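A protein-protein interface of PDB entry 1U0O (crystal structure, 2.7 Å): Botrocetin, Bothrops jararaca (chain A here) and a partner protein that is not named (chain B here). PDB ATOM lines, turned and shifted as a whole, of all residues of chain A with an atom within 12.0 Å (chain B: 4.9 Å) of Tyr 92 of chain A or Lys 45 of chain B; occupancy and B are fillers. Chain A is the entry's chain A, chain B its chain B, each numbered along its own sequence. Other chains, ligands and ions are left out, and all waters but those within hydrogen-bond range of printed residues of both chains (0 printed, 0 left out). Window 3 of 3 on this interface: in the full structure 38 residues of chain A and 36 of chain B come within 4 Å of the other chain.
OD1 of Asn 106 of chain B sits at hydrogen-bond distance from OH of Tyr 92 of chain A, 3.5 Å away. O of Asn 106 of chain B lies close to ND2 of Asn 94 of chain A. O of Asn 94 of chain A lies within hydrogen-bond range of N of Trp 108 of chain B, at 3.3 Å. O of Trp 108 of chain B is in hydrogen-bond range of N of Val 96 of chain A, at 2.6 Å.
NZ of Lys 78 of chain A is in salt-bridge range of OE1 of Glu 93 of chain A (3.1 Å). NZ of Lys 78 of chain A is in hydrogen-bond range of O of Val 95 of chain A, 2.8 Å away. The side-chain amide oxygen (OD1) of Asn 94 of chain A lies within hydrogen-bond range of the side-chain hydroxyl (OH) of Tyr 92 of chain A. The side-chain carboxylate of Glu 93 of chain A is in hydrogen-bond range of the backbone NH of Val 95 of chain A, 2.9 Å away. The side-chain carboxylate (OE2) of Glu 47 of chain B is in hydrogen-bond range of the backbone NH (N) of Gln 43 of chain B (2.7 Å).
Among the printed residues, pairs that only touch across the chains: Trp 84 of chain A with Phe 42 of chain B (3.6 Å), Trp 84 of chain A with Trp 108 of chain B (3.1 Å), Ser 89 of chain A with Gln 43 of chain B (3.8 Å), Tyr 92 of chain A with Phe 42 of chain B (3.0 Å), Tyr 92 of chain A with Gln 43 of chain B (2.8 Å), Tyr 92 of chain A with Ser 44 of chain B (3.2 Å), Tyr 92 of chain A with Lys 45 of chain B (3.1 Å), Tyr 92 of chain A with Trp 108 of chain B (3.2 Å), Glu 93 of chain A with Trp 108 of chain B (3.3 Å) and Val 95 of chain A with Trp 108 of chain B (3.4 Å).
Tyr 92 of chain A touches just these residues of chain B: Phe 42, Gln 43, Ser 44, Lys 45, Asn 106 and Trp 108. Phe 42 of chain B touches two residues of chain A. No residue of chain A comes within 4 Å of Asp 49 of chain B. Of the printed residues of chain B, Val 96 of chain A touches Trp 108. Of the printed residues of chain B, Asn 94 of chain A touches Asn 106 (3.2 Å) and Trp 108 (3.3 Å). Printed residues of chain B within 4 Å of Val 95 of chain A: Trp 108. Printed residues of chain B within 4 Å of Ser 89 of chain A: Gln 43 (3.8 Å). Of the printed residues of chain A, Trp 108 of chain B touches Trp 84 (3.1 Å), Tyr 92 (3.2 Å), Glu 93 (3.3 Å), Asn 94 (3.3 Å), Val 95 (3.4 Å) and Val 96 (2.6 Å). Ser 81 of chain A touches none of the printed residues of chain B. Gly 87 of chain A touches none of the printed residues of chain B. The nearest printed residue of chain A that does not touch Asn 106 of chain B is Val 95 of chain A (6.5 Å).
Hydrophobic or aromatic side chains of chain B within 4 Å of the printed part of chain A: Trp 108. Of the 20 printed residues of chain A, 7 touch a printed residue of chain B. Printed residues of chain A that touch a printed residue of chain B: Trp 84, Ser 89, Tyr 92, Glu 93, Asn 94, Val 95 and Val 96.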
ATOM      1  N   GLU A  77       7.354  21.156  13.584  1.00  0.00           N
ATOM      2  CA  GLU A  77       8.654  21.021  12.939  1.00  0.00           C
ATOM      3  C   GLU A  77       9.019  19.556  13.220  1.00  0.00           C
ATOM      4  O   GLU A  77       8.359  18.903  14.027  1.00  0.00           O
ATOM      5  CB  GLU A  77       9.701  21.958  13.562  1.00  0.00           C
ATOM      6  CG  GLU A  77       9.318  23.438  13.621  1.00  0.00           C
ATOM      7  CD  GLU A  77       8.391  23.764  14.799  1.00  0.00           C
ATOM      8  OE1 GLU A  77       8.776  23.492  15.967  1.00  0.00           O
ATOM      9  OE2 GLU A  77       7.282  24.299  14.554  1.00  0.00           O
ATOM     10  N   LYS A  78      10.051  19.029  12.573  1.00  0.00           N
ATOM     11  CA  LYS A  78      10.400  17.631  12.803  1.00  0.00           C
ATOM     12  C   LYS A  78      11.146  17.372  14.111  1.00  0.00           C
ATOM     13  O   LYS A  78      11.224  16.234  14.573  1.00  0.00           O
ATOM     14  CB  LYS A  78      11.183  17.069  11.602  1.00  0.00           C
ATOM     15  CG  LYS A  78      10.284  16.668  10.423  1.00  0.00           C
ATOM     16  CD  LYS A  78      11.076  16.121   9.245  1.00  0.00           C
ATOM     17  CE  LYS A  78      11.943  17.213   8.605  1.00  0.00           C
ATOM     18  NZ  LYS A  78      12.864  16.702   7.540  1.00  0.00           N
ATOM     19  N   GLN A  79      11.691  18.426  14.702  1.00  0.00           N
ATOM     20  CA  GLN A  79      12.405  18.319  15.968  1.00  0.00           C
ATOM     21  C   GLN A  79      12.168  19.649  16.687  1.00  0.00           C
ATOM     22  O   GLN A  79      11.750  20.612  16.053  1.00  0.00           O
ATOM     23  CB  GLN A  79      13.896  18.034  15.716  1.00  0.00           C
ATOM     24  CG  GLN A  79      14.688  19.145  15.073  1.00  0.00           C
ATOM     25  CD  GLN A  79      15.161  20.164  16.086  1.00  0.00           C
ATOM     26  OE1 GLN A  79      15.754  19.808  17.098  1.00  0.00           O
ATOM     27  NE2 GLN A  79      14.907  21.439  15.818  1.00  0.00           N
ATOM     28  N   CYS A  80      12.419  19.727  17.989  1.00  0.00           N
ATOM     29  CA  CYS A  80      12.139  20.967  18.694  1.00  0.00           C
ATOM     30  C   CYS A  80      13.280  21.850  19.174  1.00  0.00           C
ATOM     31  O   CYS A  80      13.061  22.786  19.939  1.00  0.00           O
ATOM     32  CB  CYS A  80      11.221  20.668  19.865  1.00  0.00           C
ATOM     33  SG  CYS A  80       9.784  19.669  19.389  1.00  0.00           S
ATOM     34  N   SER A  81      14.500  21.570  18.740  1.00  0.00           N
ATOM     35  CA  SER A  81      15.632  22.396  19.153  1.00  0.00           C
ATOM     36  C   SER A  81      15.640  23.587  18.209  1.00  0.00           C
ATOM     37  O   SER A  81      15.894  23.419  17.025  1.00  0.00           O
ATOM     38  CB  SER A  81      16.940  21.609  19.022  1.00  0.00           C
ATOM     39  OG  SER A  81      18.019  22.284  19.643  1.00  0.00           O
ATOM     40  N   SER A  82      15.357  24.784  18.720  1.00  0.00           N
ATOM     41  CA  SER A  82      15.322  25.980  17.876  1.00  0.00           C
ATOM     42  C   SER A  82      16.666  26.705  17.747  1.00  0.00           C
ATOM     43  O   SER A  82      16.754  27.765  17.127  1.00  0.00           O
ATOM     44  CB  SER A  82      14.267  26.964  18.397  1.00  0.00           C
ATOM     45  OG  SER A  82      14.837  27.914  19.277  1.00  0.00           O
ATOM     46  N   GLU A  83      17.712  26.143  18.333  1.00  0.00           N
ATOM     47  CA  GLU A  83      19.028  26.757  18.246  1.00  0.00           C
ATOM     48  C   GLU A  83      20.116  25.700  18.264  1.00  0.00           C
ATOM     49  O   GLU A  83      19.991  24.678  18.944  1.00  0.00           O
ATOM     50  CB  GLU A  83      19.275  27.707  19.420  1.00  0.00           C
ATOM     51  CG  GLU A  83      18.216  28.760  19.631  1.00  0.00           C
ATOM     52  CD  GLU A  83      18.637  29.806  20.657  1.00  0.00           C
ATOM     53  OE1 GLU A  83      19.540  30.616  20.347  1.00  0.00           O
ATOM     54  OE2 GLU A  83      18.070  29.812  21.775  1.00  0.00           O
ATOM     55  N   TRP A  84      21.186  25.938  17.516  1.00  0.00           N
ATOM     56  CA  TRP A  84      22.283  24.996  17.531  1.00  0.00           C
ATOM     57  C   TRP A  84      23.016  25.207  18.852  1.00  0.00           C
ATOM     58  O   TRP A  84      22.682  26.123  19.603  1.00  0.00           O
ATOM     59  CB  TRP A  84      23.208  25.227  16.330  1.00  0.00           C
ATOM     60  CG  TRP A  84      22.553  24.848  15.025  1.00  0.00           C
ATOM     61  CD1 TRP A  84      21.624  25.570  14.345  1.00  0.00           C
ATOM     62  CD2 TRP A  84      22.724  23.621  14.291  1.00  0.00           C
ATOM     63  NE1 TRP A  84      21.201  24.878  13.236  1.00  0.00           N
ATOM     64  CE2 TRP A  84      21.860  23.677  13.178  1.00  0.00           C
ATOM     65  CE3 TRP A  84      23.521  22.480  14.466  1.00  0.00           C
ATOM     66  CZ2 TRP A  84      21.774  22.636  12.242  1.00  0.00           C
ATOM     67  CZ3 TRP A  84      23.434  21.448  13.530  1.00  0.00           C
ATOM     68  CH2 TRP A  84      22.569  21.536  12.438  1.00  0.00           C
ATOM     69  N   SER A  85      23.993  24.364  19.159  1.00  0.00           N
ATOM     70  CA  SER A  85      24.726  24.517  20.403  1.00  0.00           C
ATOM     71  C   SER A  85      25.543  25.799  20.452  1.00  0.00           C
ATOM     72  O   SER A  85      26.051  26.164  21.508  1.00  0.00           O
ATOM     73  CB  SER A  85      25.654  23.326  20.622  1.00  0.00           C
ATOM     74  OG  SER A  85      26.558  23.193  19.547  1.00  0.00           O
ATOM     75  N   ASP A  86      25.674  26.476  19.309  1.00  0.00           N
ATOM     76  CA  ASP A  86      26.452  27.718  19.222  1.00  0.00           C
ATOM     77  C   ASP A  86      25.586  28.974  19.305  1.00  0.00           C
ATOM     78  O   ASP A  86      26.070  30.082  19.084  1.00  0.00           O
ATOM     79  CB  ASP A  86      27.271  27.751  17.923  1.00  0.00           C
ATOM     80  CG  ASP A  86      26.404  27.796  16.675  1.00  0.00           C
ATOM     81  OD1 ASP A  86      25.168  27.814  16.799  1.00  0.00           O
ATOM     82  OD2 ASP A  86      26.960  27.813  15.557  1.00  0.00           O
ATOM     83  N   GLY A  87      24.309  28.789  19.631  1.00  0.00           N
ATOM     84  CA  GLY A  87      23.394  29.910  19.743  1.00  0.00           C
ATOM     85  C   GLY A  87      22.728  30.246  18.428  1.00  0.00           C
ATOM     86  O   GLY A  87      21.694  30.900  18.398  1.00  0.00           O
ATOM     87  N   SER A  88      23.327  29.802  17.332  1.00  0.00           N
ATOM     88  CA  SER A  88      22.782  30.072  16.009  1.00  0.00           C
ATOM     89  C   SER A  88      21.369  29.508  15.904  1.00  0.00           C
ATOM     90  O   SER A  88      21.084  28.438  16.437  1.00  0.00           O
ATOM     91  CB  SER A  88      23.671  29.430  14.940  1.00  0.00           C
ATOM     92  OG  SER A  88      25.045  29.689  15.192  1.00  0.00           O
ATOM     93  N   SER A  89      20.492  30.225  15.211  1.00  0.00           N
ATOM     94  CA  SER A  89      19.107  29.806  15.034  1.00  0.00           C
ATOM     95  C   SER A  89      19.008  28.579  14.137  1.00  0.00           C
ATOM     96  O   SER A  89      19.832  28.382  13.246  1.00  0.00           O
ATOM     97  CB  SER A  89      18.299  30.942  14.407  1.00  0.00           C
ATOM     98  OG  SER A  89      18.629  32.182  15.005  1.00  0.00           O
ATOM     99  N   VAL A  90      17.991  27.756  14.379  1.00  0.00           N
ATOM    100  CA  VAL A  90      17.767  26.552  13.582  1.00  0.00           C
ATOM    101  C   VAL A  90      16.690  26.802  12.538  1.00  0.00           C
ATOM    102  O   VAL A  90      15.495  26.787  12.847  1.00  0.00           O
ATOM    103  CB  VAL A  90      17.322  25.361  14.450  1.00  0.00           C
ATOM    104  CG1 VAL A  90      16.721  24.271  13.569  1.00  0.00           C
ATOM    105  CG2 VAL A  90      18.510  24.822  15.239  1.00  0.00           C
ATOM    106  N   SER A  91      17.123  27.033  11.304  1.00  0.00           N
ATOM    107  CA  SER A  91      16.211  27.285  10.195  1.00  0.00           C
ATOM    108  C   SER A  91      16.247  26.080   9.266  1.00  0.00           C
ATOM    109  O   SER A  91      15.256  25.357   9.094  1.00  0.00           O
ATOM    110  CB  SER A  91      16.670  28.533   9.449  1.00  0.00           C
ATOM    111  OG  SER A  91      18.080  28.520   9.292  1.00  0.00           O
ATOM    112  N   TYR A  92      17.427  25.893   8.687  1.00  0.00           N
ATOM    113  CA  TYR A  92      17.752  24.812   7.768  1.00  0.00           C
ATOM    114  C   TYR A  92      17.876  23.487   8.530  1.00  0.00           C
ATOM    115  O   TYR A  92      18.504  23.425   9.584  1.00  0.00           O
ATOM    116  CB  TYR A  92      19.076  25.171   7.094  1.00  0.00           C
ATOM    117  CG  TYR A  92      19.671  24.132   6.188  1.00  0.00           C
ATOM    118  CD1 TYR A  92      18.895  23.508   5.217  1.00  0.00           C
ATOM    119  CD2 TYR A  92      21.026  23.819   6.255  1.00  0.00           C
ATOM    120  CE1 TYR A  92      19.453  22.602   4.330  1.00  0.00           C
ATOM    121  CE2 TYR A  92      21.593  22.913   5.371  1.00  0.00           C
ATOM    122  CZ  TYR A  92      20.798  22.310   4.409  1.00  0.00           C
ATOM    123  OH  TYR A  92      21.333  21.419   3.512  1.00  0.00           O
ATOM    124  N   GLU A  93      17.262  22.434   8.002  1.00  0.00           N
ATOM    125  CA  GLU A  93      17.315  21.120   8.630  1.00  0.00           C
ATOM    126  C   GLU A  93      17.124  20.015   7.595  1.00  0.00           C
ATOM    127  O   GLU A  93      16.712  20.276   6.460  1.00  0.00           O
ATOM    128  CB  GLU A  93      16.259  21.012   9.732  1.00  0.00           C
ATOM    129  CG  GLU A  93      14.833  21.176   9.254  1.00  0.00           C
ATOM    130  CD  GLU A  93      14.319  19.954   8.520  1.00  0.00           C
ATOM    131  OE1 GLU A  93      14.484  18.837   9.054  1.00  0.00           O
ATOM    132  OE2 GLU A  93      13.750  20.106   7.420  1.00  0.00           O
ATOM    133  N   ASN A  94      17.429  18.786   7.997  1.00  0.00           N
ATOM    134  CA  ASN A  94      17.327  17.623   7.121  1.00  0.00           C
ATOM    135  C   ASN A  94      16.838  16.375   7.848  1.00  0.00           C
ATOM    136  O   ASN A  94      16.965  15.265   7.346  1.00  0.00           O
ATOM    137  CB  ASN A  94      18.690  17.316   6.515  1.00  0.00           C
ATOM    138  CG  ASN A  94      18.804  17.768   5.097  1.00  0.00           C
ATOM    139  OD1 ASN A  94      19.501  18.731   4.800  1.00  0.00           O
ATOM    140  ND2 ASN A  94      18.113  17.077   4.204  1.00  0.00           N
ATOM    141  N   VAL A  95      16.287  16.551   9.036  1.00  0.00           N
ATOM    142  CA  VAL A  95      15.806  15.417   9.802  1.00  0.00           C
ATOM    143  C   VAL A  95      15.251  14.260   8.943  1.00  0.00           C
ATOM    144  O   VAL A  95      14.465  14.457   8.021  1.00  0.00           O
ATOM    145  CB  VAL A  95      14.751  15.888  10.827  1.00  0.00           C
ATOM    146  CG1 VAL A  95      14.127  14.696  11.527  1.00  0.00           C
ATOM    147  CG2 VAL A  95      15.405  16.811  11.843  1.00  0.00           C
ATOM    148  N   VAL A  96      15.717  13.056   9.250  1.00  0.00           N
ATOM    149  CA  VAL A  96      15.292  11.827   8.588  1.00  0.00           C
ATOM    150  C   VAL A  96      13.947  11.498   9.215  1.00  0.00           C
ATOM    151  O   VAL A  96      13.870  10.926  10.291  1.00  0.00           O
ATOM    152  CB  VAL A  96      16.305  10.680   8.873  1.00  0.00           C
ATOM    153  CG1 VAL A  96      15.657   9.312   8.675  1.00  0.00           C
ATOM    154  CG2 VAL A  96      17.512  10.834   7.965  1.00  0.00           C
ATOM    155  N   PHE B  42      24.842  23.581  10.511  1.00  0.00           N
ATOM    156  CA  PHE B  42      24.605  23.793   9.085  1.00  0.00           C
ATOM    157  C   PHE B  42      23.507  24.817   8.788  1.00  0.00           C
ATOM    158  O   PHE B  42      22.321  24.534   8.918  1.00  0.00           O
ATOM    159  CB  PHE B  42      24.256  22.463   8.409  1.00  0.00           C
ATOM    160  CG  PHE B  42      25.380  21.455   8.417  1.00  0.00           C
ATOM    161  CD1 PHE B  42      25.116  20.099   8.245  1.00  0.00           C
ATOM    162  CD2 PHE B  42      26.701  21.857   8.580  1.00  0.00           C
ATOM    163  CE1 PHE B  42      26.152  19.159   8.237  1.00  0.00           C
ATOM    164  CE2 PHE B  42      27.741  20.920   8.572  1.00  0.00           C
ATOM    165  CZ  PHE B  42      27.464  19.573   8.401  1.00  0.00           C
ATOM    166  N   GLN B  43      23.930  26.006   8.372  1.00  0.00           N
ATOM    167  CA  GLN B  43      23.038  27.114   8.034  1.00  0.00           C
ATOM    168  C   GLN B  43      22.426  26.907   6.648  1.00  0.00           C
ATOM    169  O   GLN B  43      21.208  26.944   6.480  1.00  0.00           O
ATOM    170  CB  GLN B  43      23.832  28.419   8.038  1.00  0.00           C
ATOM    171  CG  GLN B  43      24.622  28.658   9.311  1.00  0.00           C
ATOM    172  CD  GLN B  43      23.751  29.121  10.459  1.00  0.00           C
ATOM    173  OE1 GLN B  43      22.778  28.451  10.832  1.00  0.00           O
ATOM    174  NE2 GLN B  43      24.094  30.279  11.031  1.00  0.00           N
ATOM    175  N   SER B  44      23.297  26.707   5.661  1.00  0.00           N
ATOM    176  CA  SER B  44      22.903  26.481   4.268  1.00  0.00           C
ATOM    177  C   SER B  44      23.412  25.107   3.806  1.00  0.00           C
ATOM    178  O   SER B  44      24.216  24.470   4.501  1.00  0.00           O
ATOM    179  CB  SER B  44      23.506  27.573   3.384  1.00  0.00           C
ATOM    180  OG  SER B  44      24.890  27.716   3.654  1.00  0.00           O
ATOM    181  N   LYS B  45      22.953  24.653   2.640  1.00  0.00           N
ATOM    182  CA  LYS B  45      23.385  23.359   2.121  1.00  0.00           C
ATOM    183  C   LYS B  45      24.859  23.389   1.722  1.00  0.00           C
ATOM    184  O   LYS B  45      25.565  22.392   1.866  1.00  0.00           O
ATOM    185  CB  LYS B  45      22.544  22.954   0.918  1.00  0.00           C
ATOM    186  CG  LYS B  45      22.969  21.630   0.307  1.00  0.00           C
ATOM    187  CD  LYS B  45      22.192  21.322  -0.967  1.00  0.00           C
ATOM    188  CE  LYS B  45      22.711  20.060  -1.648  1.00  0.00           C
ATOM    189  NZ  LYS B  45      21.946  19.769  -2.893  1.00  0.00           N
ATOM    190  N   GLU B  46      25.316  24.538   1.227  1.00  0.00           N
ATOM    191  CA  GLU B  46      26.707  24.701   0.816  1.00  0.00           C
ATOM    192  C   GLU B  46      27.641  24.382   1.970  1.00  0.00           C
ATOM    193  O   GLU B  46      28.643  23.688   1.786  1.00  0.00           O
ATOM    194  CB  GLU B  46      26.973  26.129   0.315  1.00  0.00           C
ATOM    195  CG  GLU B  46      26.376  26.435  -1.062  1.00  0.00           C
ATOM    196  CD  GLU B  46      24.855  26.553  -1.047  1.00  0.00           C
ATOM    197  OE1 GLU B  46      24.230  26.369  -2.118  1.00  0.00           O
ATOM    198  OE2 GLU B  46      24.284  26.842   0.029  1.00  0.00           O
ATOM    199  N   GLU B  47      27.303  24.887   3.158  1.00  0.00           N
ATOM    200  CA  GLU B  47      28.105  24.653   4.361  1.00  0.00           C
ATOM    201  C   GLU B  47      28.190  23.156   4.557  1.00  0.00           C
ATOM    202  O   GLU B  47      29.272  22.596   4.730  1.00  0.00           O
ATOM    203  CB  GLU B  47      27.440  25.292   5.582  1.00  0.00           C
ATOM    204  CG  GLU B  47      28.243  25.181   6.868  1.00  0.00           C
ATOM    205  CD  GLU B  47      27.619  25.963   8.013  1.00  0.00           C
ATOM    206  OE1 GLU B  47      28.224  26.045   9.105  1.00  0.00           O
ATOM    207  OE2 GLU B  47      26.513  26.501   7.823  1.00  0.00           O
ATOM    208  N   ALA B  48      27.027  22.516   4.514  1.00  0.00           N
ATOM    209  CA  ALA B  48      26.919  21.076   4.668  1.00  0.00           C
ATOM    210  C   ALA B  48      27.890  20.371   3.731  1.00  0.00           C
ATOM    211  O   ALA B  48      28.757  19.615   4.170  1.00  0.00           O
ATOM    212  CB  ALA B  48      25.492  20.640   4.372  1.00  0.00           C
ATOM    213  N   ASP B  49      27.735  20.635   2.438  1.00  0.00           N
ATOM    214  CA  ASP B  49      28.573  20.044   1.397  1.00  0.00           C
ATOM    215  C   ASP B  49      30.058  20.271   1.668  1.00  0.00           C
ATOM    216  O   ASP B  49      30.894  19.424   1.353  1.00  0.00           O
ATOM    217  CB  ASP B  49      28.184  20.633   0.037  1.00  0.00           C
ATOM    218  CG  ASP B  49      26.754  20.275  -0.377  1.00  0.00           C
ATOM    219  OD1 ASP B  49      26.186  21.012  -1.214  1.00  0.00           O
ATOM    220  OD2 ASP B  49      26.198  19.260   0.118  1.00  0.00           O
ATOM    221  N   ASN B 106      23.706  13.818   3.360  1.00  0.00           N
ATOM    222  CA  ASN B 106      23.392  14.906   4.281  1.00  0.00           C
ATOM    223  C   ASN B 106      21.998  14.750   4.880  1.00  0.00           C
ATOM    224  O   ASN B 106      21.188  15.666   4.832  1.00  0.00           O
ATOM    225  CB  ASN B 106      23.499  16.282   3.603  1.00  0.00           C
ATOM    226  CG  ASN B 106      23.555  17.441   4.626  1.00  0.00           C
ATOM    227  OD1 ASN B 106      23.044  18.537   4.376  1.00  0.00           O
ATOM    228  ND2 ASN B 106      24.194  17.194   5.774  1.00  0.00           N
ATOM    229  N   TRP B 108      19.907  14.088   8.294  1.00  0.00           N
ATOM    230  CA  TRP B 108      20.061  14.194   9.730  1.00  0.00           C
ATOM    231  C   TRP B 108      19.313  13.097  10.450  1.00  0.00           C
ATOM    232  O   TRP B 108      18.137  12.855  10.183  1.00  0.00           O
ATOM    233  CB  TRP B 108      19.552  15.548  10.199  1.00  0.00           C
ATOM    234  CG  TRP B 108      20.290  16.699   9.600  1.00  0.00           C
ATOM    235  CD1 TRP B 108      21.273  16.648   8.648  1.00  0.00           C
ATOM    236  CD2 TRP B 108      20.133  18.075   9.942  1.00  0.00           C
ATOM    237  NE1 TRP B 108      21.740  17.914   8.381  1.00  0.00           N
ATOM    238  CE2 TRP B 108      21.057  18.808   9.163  1.00  0.00           C
ATOM    239  CE3 TRP B 108      19.302  18.763  10.836  1.00  0.00           C
ATOM    240  CZ2 TRP B 108      21.174  20.190   9.253  1.00  0.00           C
ATOM    241  CZ3 TRP B 108      19.421  20.143  10.925  1.00  0.00           C
ATOM    242  CH2 TRP B 108      20.349  20.838  10.138  1.00  0.00           C
